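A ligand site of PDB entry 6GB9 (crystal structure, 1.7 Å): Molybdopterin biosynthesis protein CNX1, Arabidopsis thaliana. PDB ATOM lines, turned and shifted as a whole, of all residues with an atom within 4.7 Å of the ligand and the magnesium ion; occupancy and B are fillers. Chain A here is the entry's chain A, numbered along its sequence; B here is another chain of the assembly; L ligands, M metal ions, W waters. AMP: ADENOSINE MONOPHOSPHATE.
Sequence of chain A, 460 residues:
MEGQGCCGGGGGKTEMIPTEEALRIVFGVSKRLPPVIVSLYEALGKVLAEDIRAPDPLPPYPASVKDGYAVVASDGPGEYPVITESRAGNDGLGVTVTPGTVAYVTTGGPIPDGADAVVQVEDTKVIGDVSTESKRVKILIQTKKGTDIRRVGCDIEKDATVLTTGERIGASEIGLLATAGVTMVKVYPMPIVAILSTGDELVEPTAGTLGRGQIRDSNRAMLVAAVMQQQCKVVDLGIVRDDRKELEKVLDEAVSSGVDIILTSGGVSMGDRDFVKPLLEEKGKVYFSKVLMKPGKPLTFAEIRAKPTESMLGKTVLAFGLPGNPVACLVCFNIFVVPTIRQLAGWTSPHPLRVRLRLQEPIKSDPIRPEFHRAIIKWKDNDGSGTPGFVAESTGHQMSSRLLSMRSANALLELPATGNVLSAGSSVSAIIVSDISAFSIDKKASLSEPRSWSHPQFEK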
ATOM      1  N   SER A 197      12.184   1.575 -20.638  1.00  0.00           N
ATOM      2  CA  SER A 197      12.006   2.585 -19.597  1.00  0.00           C
ATOM      3  C   SER A 197      13.229   2.510 -18.712  1.00  0.00           C
ATOM      4  O   SER A 197      13.878   1.468 -18.625  1.00  0.00           O
ATOM      5  CB  SER A 197      10.748   2.295 -18.772  1.00  0.00           C
ATOM      6  OG  SER A 197       9.624   2.652 -19.561  1.00  0.00           O
ATOM      7  N   THR A 198      13.498   3.607 -18.018  1.00  0.00           N
ATOM      8  CA  THR A 198      14.616   3.686 -17.095  1.00  0.00           C
ATOM      9  C   THR A 198      14.154   4.188 -15.744  1.00  0.00           C
ATOM     10  O   THR A 198      13.338   5.104 -15.647  1.00  0.00           O
ATOM     11  CB  THR A 198      15.785   4.569 -17.634  1.00  0.00           C
ATOM     12  OG1 THR A 198      15.459   5.967 -17.549  1.00  0.00           O
ATOM     13  CG2 THR A 198      16.228   4.168 -19.049  1.00  0.00           C
ATOM     14  N   GLY A 199      14.723   3.605 -14.704  1.00  0.00           N
ATOM     15  CA  GLY A 199      14.515   4.095 -13.347  1.00  0.00           C
ATOM     16  C   GLY A 199      14.497   3.072 -12.243  1.00  0.00           C
ATOM     17  O   GLY A 199      13.740   2.107 -12.294  1.00  0.00           O
ATOM     18  N   GLU A 201      13.068   3.737  -9.449  1.00  0.00           N
ATOM     19  CA  GLU A 201      11.757   3.939  -8.820  1.00  0.00           C
ATOM     20  C   GLU A 201      10.635   3.174  -9.540  1.00  0.00           C
ATOM     21  O   GLU A 201       9.519   3.089  -9.031  1.00  0.00           O
ATOM     22  CB  GLU A 201      11.396   5.458  -8.707  1.00  0.00           C
ATOM     23  CG  GLU A 201      10.840   6.141  -9.957  1.00  0.00           C
ATOM     24  CD  GLU A 201      11.832   6.474 -11.060  1.00  0.00           C
ATOM     25  OE1 GLU A 201      12.967   5.946 -11.048  1.00  0.00           O
ATOM     26  OE2 GLU A 201      11.458   7.258 -11.956  1.00  0.00           O
ATOM     27  N   LEU A 202      10.906   2.663 -10.729  1.00  0.00           N
ATOM     28  CA  LEU A 202       9.834   2.001 -11.486  1.00  0.00           C
ATOM     29  C   LEU A 202       9.553   0.577 -11.059  1.00  0.00           C
ATOM     30  O   LEU A 202      10.477  -0.161 -10.712  1.00  0.00           O
ATOM     31  CB  LEU A 202      10.188   1.971 -12.993  1.00  0.00           C
ATOM     32  CG  LEU A 202      10.508   3.328 -13.674  1.00  0.00           C
ATOM     33  CD1 LEU A 202      10.849   3.098 -15.157  1.00  0.00           C
ATOM     34  CD2 LEU A 202       9.332   4.315 -13.544  1.00  0.00           C
ATOM     35  N   ILE A 215       6.689   3.838  -8.402  1.00  0.00           N
ATOM     36  CA  ILE A 215       5.610   4.195  -9.288  1.00  0.00           C
ATOM     37  C   ILE A 215       5.531   3.139 -10.364  1.00  0.00           C
ATOM     38  O   ILE A 215       6.554   2.528 -10.718  1.00  0.00           O
ATOM     39  CB  ILE A 215       5.747   5.600  -9.927  1.00  0.00           C
ATOM     40  CG1 ILE A 215       7.060   5.734 -10.779  1.00  0.00           C
ATOM     41  CG2 ILE A 215       5.681   6.677  -8.861  1.00  0.00           C
ATOM     42  CD1 ILE A 215       7.107   6.972 -11.682  1.00  0.00           C
ATOM     43  N   ARG A 216       4.355   2.964 -10.958  1.00  0.00           N
ATOM     44  CA  ARG A 216       4.234   2.028 -12.069  1.00  0.00           C
ATOM     45  C   ARG A 216       4.860   2.625 -13.320  1.00  0.00           C
ATOM     46  O   ARG A 216       4.690   3.814 -13.615  1.00  0.00           O
ATOM     47  CB  ARG A 216       2.758   1.646 -12.347  1.00  0.00           C
ATOM     48  CG  ARG A 216       2.194   0.835 -11.178  1.00  0.00           C
ATOM     49  CD  ARG A 216       0.794   0.261 -11.405  1.00  0.00           C
ATOM     50  NE  ARG A 216       0.283  -0.203 -10.115  1.00  0.00           N
ATOM     51  CZ  ARG A 216      -0.318   0.554  -9.196  1.00  0.00           C
ATOM     52  NH1 ARG A 216      -0.577   1.841  -9.445  1.00  0.00           N
ATOM     53  NH2 ARG A 216      -0.684   0.029  -8.031  1.00  0.00           N
ATOM     54  N   ASP A 217       5.583   1.789 -14.068  1.00  0.00           N
ATOM     55  CA  ASP A 217       6.125   2.209 -15.360  1.00  0.00           C
ATOM     56  C   ASP A 217       4.899   2.463 -16.313  1.00  0.00           C
ATOM     57  O   ASP A 217       4.188   1.521 -16.658  1.00  0.00           O
ATOM     58  CB  ASP A 217       6.982   1.068 -15.941  1.00  0.00           C
ATOM     59  CG  ASP A 217       7.546   1.305 -17.316  1.00  0.00           C
ATOM     60  OD1 ASP A 217       7.340   2.407 -17.864  1.00  0.00           O
ATOM     61  OD2 ASP A 217       8.185   0.403 -17.844  1.00  0.00           O
ATOM     62  N   SER A 218       4.610   3.730 -16.634  1.00  0.00           N
ATOM     63  CA  SER A 218       3.503   4.054 -17.544  1.00  0.00           C
ATOM     64  C   SER A 218       4.025   4.422 -18.947  1.00  0.00           C
ATOM     65  O   SER A 218       3.345   4.183 -19.948  1.00  0.00           O
ATOM     66  CB  SER A 218       2.620   5.156 -16.965  1.00  0.00           C
ATOM     67  OG  SER A 218       3.326   6.373 -16.813  1.00  0.00           O
ATOM     68  N   ASN A 219       5.216   5.016 -19.051  1.00  0.00           N
ATOM     69  CA  ASN A 219       5.761   5.427 -20.342  1.00  0.00           C
ATOM     70  C   ASN A 219       5.958   4.294 -21.325  1.00  0.00           C
ATOM     71  O   ASN A 219       5.714   4.497 -22.516  1.00  0.00           O
ATOM     72  CB  ASN A 219       7.093   6.160 -20.185  1.00  0.00           C
ATOM     73  CG  ASN A 219       7.021   7.547 -19.578  1.00  0.00           C
ATOM     74  OD1 ASN A 219       5.949   8.113 -19.370  1.00  0.00           O
ATOM     75  ND2 ASN A 219       8.165   8.115 -19.253  1.00  0.00           N
ATOM     76  N   ARG A 220       6.433   3.120 -20.862  1.00  0.00           N
ATOM     77  CA  ARG A 220       6.671   2.036 -21.809  1.00  0.00           C
ATOM     78  C   ARG A 220       5.394   1.588 -22.500  1.00  0.00           C
ATOM     79  O   ARG A 220       5.365   1.594 -23.730  1.00  0.00           O
ATOM     80  CB  ARG A 220       7.376   0.852 -21.128  1.00  0.00           C
ATOM     81  CG  ARG A 220       7.825  -0.267 -22.077  1.00  0.00           C
ATOM     82  CD  ARG A 220       8.937  -1.051 -21.384  1.00  0.00           C
ATOM     83  NE  ARG A 220       8.577  -1.353 -19.989  1.00  0.00           N
ATOM     84  CZ  ARG A 220       8.026  -2.484 -19.547  1.00  0.00           C
ATOM     85  NH1 ARG A 220       7.825  -3.518 -20.375  1.00  0.00           N
ATOM     86  NH2 ARG A 220       7.706  -2.591 -18.264  1.00  0.00           N
ATOM     87  N   ASP A 242      19.042   2.389 -13.084  1.00  0.00           N
ATOM     88  CA  ASP A 242      19.954   3.540 -13.215  1.00  0.00           C
ATOM     89  C   ASP A 242      21.379   3.104 -12.914  1.00  0.00           C
ATOM     90  O   ASP A 242      21.995   3.452 -11.904  1.00  0.00           O
ATOM     91  CB  ASP A 242      19.479   4.726 -12.339  1.00  0.00           C
ATOM     92  CG  ASP A 242      18.046   5.157 -12.658  1.00  0.00           C
ATOM     93  OD1 ASP A 242      17.693   5.254 -13.863  1.00  0.00           O
ATOM     94  OD2 ASP A 242      17.271   5.397 -11.720  1.00  0.00           O
ATOM     95  N   SER A 265      13.060   6.416 -22.257  1.00  0.00           N
ATOM     96  CA  SER A 265      12.459   7.550 -21.571  1.00  0.00           C
ATOM     97  C   SER A 265      13.130   7.631 -20.190  1.00  0.00           C
ATOM     98  O   SER A 265      13.576   6.615 -19.667  1.00  0.00           O
ATOM     99  CB  SER A 265      10.939   7.459 -21.481  1.00  0.00           C
ATOM    100  OG  SER A 265      10.466   6.553 -20.495  1.00  0.00           O
ATOM    101  N   GLY A 266      13.285   8.829 -19.665  1.00  0.00           N
ATOM    102  CA  GLY A 266      13.937   9.049 -18.379  1.00  0.00           C
ATOM    103  C   GLY A 266      15.451   9.016 -18.512  1.00  0.00           C
ATOM    104  O   GLY A 266      15.990   8.815 -19.595  1.00  0.00           O
ATOM    105  N   GLY A 267      16.144   9.203 -17.391  1.00  0.00           N
ATOM    106  CA  GLY A 267      17.606   9.178 -17.370  1.00  0.00           C
ATOM    107  C   GLY A 267      18.276  10.204 -18.271  1.00  0.00           C
ATOM    108  O   GLY A 267      19.399   9.964 -18.720  1.00  0.00           O
ATOM    109  N   VAL A 268      17.593  11.346 -18.548  1.00  0.00           N
ATOM    110  CA  VAL A 268      18.096  12.434 -19.416  1.00  0.00           C
ATOM    111  C   VAL A 268      17.996  13.818 -18.775  1.00  0.00           C
ATOM    112  O   VAL A 268      18.168  14.782 -19.492  1.00  0.00           O
ATOM    113  CB  VAL A 268      17.405  12.456 -20.838  1.00  0.00           C
ATOM    114  CG1 VAL A 268      17.926  11.356 -21.722  1.00  0.00           C
ATOM    115  CG2 VAL A 268      15.879  12.418 -20.737  1.00  0.00           C
ATOM    116  N   SER A 269      17.732  13.921 -17.448  1.00  0.00           N
ATOM    117  CA  SER A 269      17.672  15.229 -16.759  1.00  0.00           C
ATOM    118  C   SER A 269      19.091  15.513 -16.174  1.00  0.00           C
ATOM    119  O   SER A 269      20.096  15.094 -16.761  1.00  0.00           O
ATOM    120  CB  SER A 269      16.582  15.242 -15.683  1.00  0.00           C
ATOM    121  OG  SER A 269      15.331  14.715 -16.096  1.00  0.00           O
ATOM    122  N   ASP A 274      21.755   9.727 -14.429  1.00  0.00           N
ATOM    123  CA  ASP A 274      21.047   9.902 -15.705  1.00  0.00           C
ATOM    124  C   ASP A 274      22.099   9.595 -16.777  1.00  0.00           C
ATOM    125  O   ASP A 274      22.897  10.474 -17.124  1.00  0.00           O
ATOM    126  CB  ASP A 274      20.476  11.341 -15.806  1.00  0.00           C
ATOM    127  CG  ASP A 274      19.211  11.564 -14.978  1.00  0.00           C
ATOM    128  OD1 ASP A 274      18.704  10.591 -14.396  1.00  0.00           O
ATOM    129  OD2 ASP A 274      18.748  12.711 -14.914  1.00  0.00           O
ATOM    130  N   GLY A 324      11.539  11.680 -19.164  1.00  0.00           N
ATOM    131  CA  GLY A 324      10.796  10.765 -18.295  1.00  0.00           C
ATOM    132  C   GLY A 324       9.407  11.242 -17.940  1.00  0.00           C
ATOM    133  O   GLY A 324       8.503  10.417 -17.741  1.00  0.00           O
ATOM    134  N   ASN A 325       9.218  12.584 -17.786  1.00  0.00           N
ATOM    135  CA  ASN A 325       7.894  13.109 -17.438  1.00  0.00           C
ATOM    136  C   ASN A 325       6.867  12.639 -18.487  1.00  0.00           C
ATOM    137  O   ASN A 325       7.084  12.857 -19.677  1.00  0.00           O
ATOM    138  CB  ASN A 325       7.906  14.628 -17.327  1.00  0.00           C
ATOM    139  CG  ASN A 325       8.366  15.108 -15.971  1.00  0.00           C
ATOM    140  OD1 ASN A 325       7.871  14.667 -14.918  1.00  0.00           O
ATOM    141  ND2 ASN A 325       9.305  16.024 -15.963  1.00  0.00           N
ATOM    142  N   PRO A 326       5.810  11.896 -18.077  1.00  0.00           N
ATOM    143  CA  PRO A 326       4.858  11.320 -19.064  1.00  0.00           C
ATOM    144  C   PRO A 326       4.323  12.229 -20.170  1.00  0.00           C
ATOM    145  O   PRO A 326       4.206  11.804 -21.305  1.00  0.00           O
ATOM    146  CB  PRO A 326       3.707  10.861 -18.162  1.00  0.00           C
ATOM    147  CG  PRO A 326       4.404  10.384 -16.926  1.00  0.00           C
ATOM    148  CD  PRO A 326       5.470  11.461 -16.700  1.00  0.00           C
ATOM    149  N   THR B 107      15.152  14.053  -9.842  1.00  0.00           N
ATOM    150  CA  THR B 107      13.758  14.221 -10.243  1.00  0.00           C
ATOM    151  C   THR B 107      13.047  12.883 -10.059  1.00  0.00           C
ATOM    152  O   THR B 107      13.582  11.847 -10.441  1.00  0.00           O
ATOM    153  CB  THR B 107      13.656  14.711 -11.692  1.00  0.00           C
ATOM    154  OG1 THR B 107      14.434  15.908 -11.823  1.00  0.00           O
ATOM    155  CG2 THR B 107      12.197  14.950 -12.128  1.00  0.00           C
ATOM    156  N   GLY B 108      11.903  12.920  -9.369  1.00  0.00           N
ATOM    157  CA  GLY B 108      11.124  11.729  -9.049  1.00  0.00           C
ATOM    158  C   GLY B 108      11.565  11.074  -7.746  1.00  0.00           C
ATOM    159  O   GLY B 108      10.930  10.119  -7.304  1.00  0.00           O
ATOM    160  N   ARG B 150       6.244  17.721  -5.823  1.00  0.00           N
ATOM    161  CA  ARG B 150       4.932  17.212  -6.215  1.00  0.00           C
ATOM    162  C   ARG B 150       4.346  16.554  -4.955  1.00  0.00           C
ATOM    163  O   ARG B 150       4.836  15.492  -4.550  1.00  0.00           O
ATOM    164  CB  ARG B 150       5.087  16.155  -7.324  1.00  0.00           C
ATOM    165  CG  ARG B 150       5.347  16.756  -8.699  1.00  0.00           C
ATOM    166  CD  ARG B 150       5.947  15.743  -9.640  1.00  0.00           C
ATOM    167  NE  ARG B 150       4.993  14.651  -9.897  1.00  0.00           N
ATOM    168  CZ  ARG B 150       5.268  13.347  -9.952  1.00  0.00           C
ATOM    169  NH1 ARG B 150       6.523  12.909  -9.769  1.00  0.00           N
ATOM    170  NH2 ARG B 150       4.306  12.459 -10.160  1.00  0.00           N
HETATM  171  P   AMP L   1      14.176  11.218 -15.023  1.00  0.00           P
HETATM  172  O1P AMP L   1      14.508  11.957 -13.726  1.00  0.00           O
HETATM  173  O2P AMP L   1      14.639   9.786 -15.024  1.00  0.00           O
HETATM  174  O3P AMP L   1      14.540  11.997 -16.244  1.00  0.00           O
HETATM  175  O5' AMP L   1      12.568  11.210 -14.985  1.00  0.00           O
HETATM  176  C5' AMP L   1      11.794  12.403 -14.867  1.00  0.00           C
HETATM  177  C4' AMP L   1      10.455  12.142 -14.195  1.00  0.00           C
HETATM  178  O4' AMP L   1       9.667  11.223 -14.971  1.00  0.00           O
HETATM  179  C3' AMP L   1      10.574  11.533 -12.811  1.00  0.00           C
HETATM  180  O3' AMP L   1       9.591  12.151 -11.973  1.00  0.00           O
HETATM  181  C2' AMP L   1      10.319  10.056 -13.031  1.00  0.00           C
HETATM  182  O2' AMP L   1       9.862   9.346 -11.879  1.00  0.00           O
HETATM  183  C1' AMP L   1       9.328  10.074 -14.190  1.00  0.00           C
HETATM  184  N9  AMP L   1       9.434   8.856 -15.001  1.00  0.00           N
HETATM  185  C8  AMP L   1      10.558   8.397 -15.594  1.00  0.00           C
HETATM  186  N7  AMP L   1      10.281   7.276 -16.289  1.00  0.00           N
HETATM  187  C5  AMP L   1       8.962   7.017 -16.163  1.00  0.00           C
HETATM  188  C6  AMP L   1       8.031   5.974 -16.633  1.00  0.00           C
HETATM  189  N6  AMP L   1       8.455   4.961 -17.376  1.00  0.00           N
HETATM  190  N1  AMP L   1       6.723   6.053 -16.287  1.00  0.00           N
HETATM  191  C2  AMP L   1       6.271   7.064 -15.509  1.00  0.00           C
HETATM  192  N3  AMP L   1       7.072   8.058 -15.049  1.00  0.00           N
HETATM  193  C4  AMP L   1       8.400   8.085 -15.353  1.00  0.00           C
HETATM  194 MG    MG M   1      14.956   8.351 -13.643  1.00  0.00          MG
HETATM  195  O   HOH W   1      13.572  13.331 -18.294  1.00  0.00           O
HETATM  196  O   HOH W   2      16.753   9.368 -13.076  1.00  0.00           O
HETATM  197  O   HOH W   3      15.191   7.132 -11.914  1.00  0.00           O
HETATM  198  O   HOH W   4       7.916  10.157  -9.764  1.00  0.00           O
HETATM  199  O   HOH W   5       7.140  12.694 -13.251  1.00  0.00           O
HETATM  200  O   HOH W   6       5.138   9.374 -13.530  1.00  0.00           O
HETATM  201  O   HOH W   7      13.842   9.454 -12.228  1.00  0.00           O
HETATM  202  O   HOH W   8      16.889  12.736 -12.966  1.00  0.00           O
HETATM  203  O   HOH W   9       9.105  14.448 -10.556  1.00  0.00           O
HETATM  204  O   HOH W  10      11.363   5.513 -18.156  1.00  0.00           O
HETATM  205  O   HOH W  11      15.924   7.054 -15.024  1.00  0.00           O
HETATM  206  O   HOH W  12      13.069   7.444 -14.066  1.00  0.00           O
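An oxygen (O2') of the ligand is in hydrogen-bond range of the side-chain carboxylate (OE2) of Glu 201 (2.6 Å). OD1 of Asp 217 sits at hydrogen-bond distance from N6 of the ligand (2.8 Å). The side-chain hydroxyl of Ser 269 lies within hydrogen-bond range of an oxygen (O3P) of the ligand (2.8 Å). N of Gly 267 sits at hydrogen-bond distance from O3P of the ligand. N of Asn 325 is in hydrogen-bond range of O4' of the ligand. A nitrogen (N1) of the ligand sits at hydrogen-bond distance from the backbone NH of Ser 218, 3.2 Å away. A nitrogen (N1) of the ligand lies close to the side-chain hydroxyl of Ser 218. The backbone NH (N) of Asn 219 sits at hydrogen-bond distance from a nitrogen (N1) of the ligand, at 3.3 Å. The side-chain hydroxyl (OG) of Ser 197 lies within hydrogen-bond range of a nitrogen (N6) of the ligand, 3.4 Å away.
The magnesium ion is bound by O2P of the ligand (2.0 Å), water W7 (2.1 Å), water W11 (2.1 Å), water W3 (2.1 Å), water W12 (2.1 Å) and water W2 (2.1 Å).
O of Glu 201 is in hydrogen-bond range of N of Ile 215 (3.0 Å). OD1 of Asp 217 sits at hydrogen-bond distance from OG of Ser 197, at 2.9 Å. The guanidinium group (NE) of Arg 220 lies within salt-bridge range of the side-chain carboxylate (OD2) of Asp 217 (2.8 Å). The side-chain hydroxyl (OG1) of Thr 198 lies within hydrogen-bond range of the backbone NH (N) of Gly 267 (3.3 Å). The side-chain amide nitrogen (ND2) of Asn 219 sits at hydrogen-bond distance from the backbone carbonyl oxygen (O) of Gly 324, at 2.8 Å. OG of Ser 265 is in hydrogen-bond range of ND2 of Asn 219 (3.0 Å). The backbone NH (N) of Arg 220 lies close to the side-chain hydroxyl (OG) of Ser 197, at 3.5 Å. OG1 of Thr 198 sits at hydrogen-bond distance from O of Ser 265 (2.9 Å).
O4' of the ligand lies close to O of Gly 324 (3.1 Å). The backbone carbonyl oxygen (O) of Thr 107 of chain B sits close to an oxygen (O1P) of the ligand. Thr 198 touches the ligand. Leu 202 touches the ligand (CD2 to C6, 3.7 Å). Ile 215 touches the ligand (CD1 to N3, 3.5 Å). Gly 266 touches the ligand (CA to O2P, 3.5 Å). Val 268 touches the ligand. Gly 108 of chain B touches the ligand (CA to O3', 3.3 Å). Arg 150 of chain B touches the ligand (NH1 to O3', 3.9 Å). Hydrophobic or aromatic side chains that line the ligand: Leu 202 and Ile 215. Within 4 Å of the ligand: Ser 197, Thr 198, Glu 201, Leu 202, Ile 215, Asp 217, Ser 218, Asn 219, Gly 266, Gly 267, Val 268, Ser 269, Gly 324, Asn 325, Thr 107 of chain B, Gly 108 of chain B and Arg 150 of chain B.
No residue comes within 4 Å of the magnesium ion.
Water W3 lies within hydrogen-bond range of OE1 of Glu 201 (2.7 Å) and OD2 of Asp 242 (2.7 Å). Water W11 lies within hydrogen-bond range of OD1 of Asp 242, OG1 of Thr 198 and N of Gly 267. Water W12 bridges the side-chain carboxylate (OE2) of Glu 201 (2.7 Å) and the backbone carbonyl oxygen (O) of Thr 198 (2.8 Å). Water W8 lies within hydrogen-bond range of an oxygen (O1P) of the ligand (2.6 Å) and the side-chain carboxylate of Asp 274 (2.7 Å). Water W1 lies within hydrogen-bond range of an oxygen (O3P) of the ligand (2.6 Å), the backbone NH of Gly 324 (2.8 Å) and the side-chain hydroxyl of Ser 269 (3.1 Å). Water W10 lies within hydrogen-bond range of the side-chain hydroxyl of Ser 265, a nitrogen (N7) of the ligand and the backbone NH of Thr 198.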
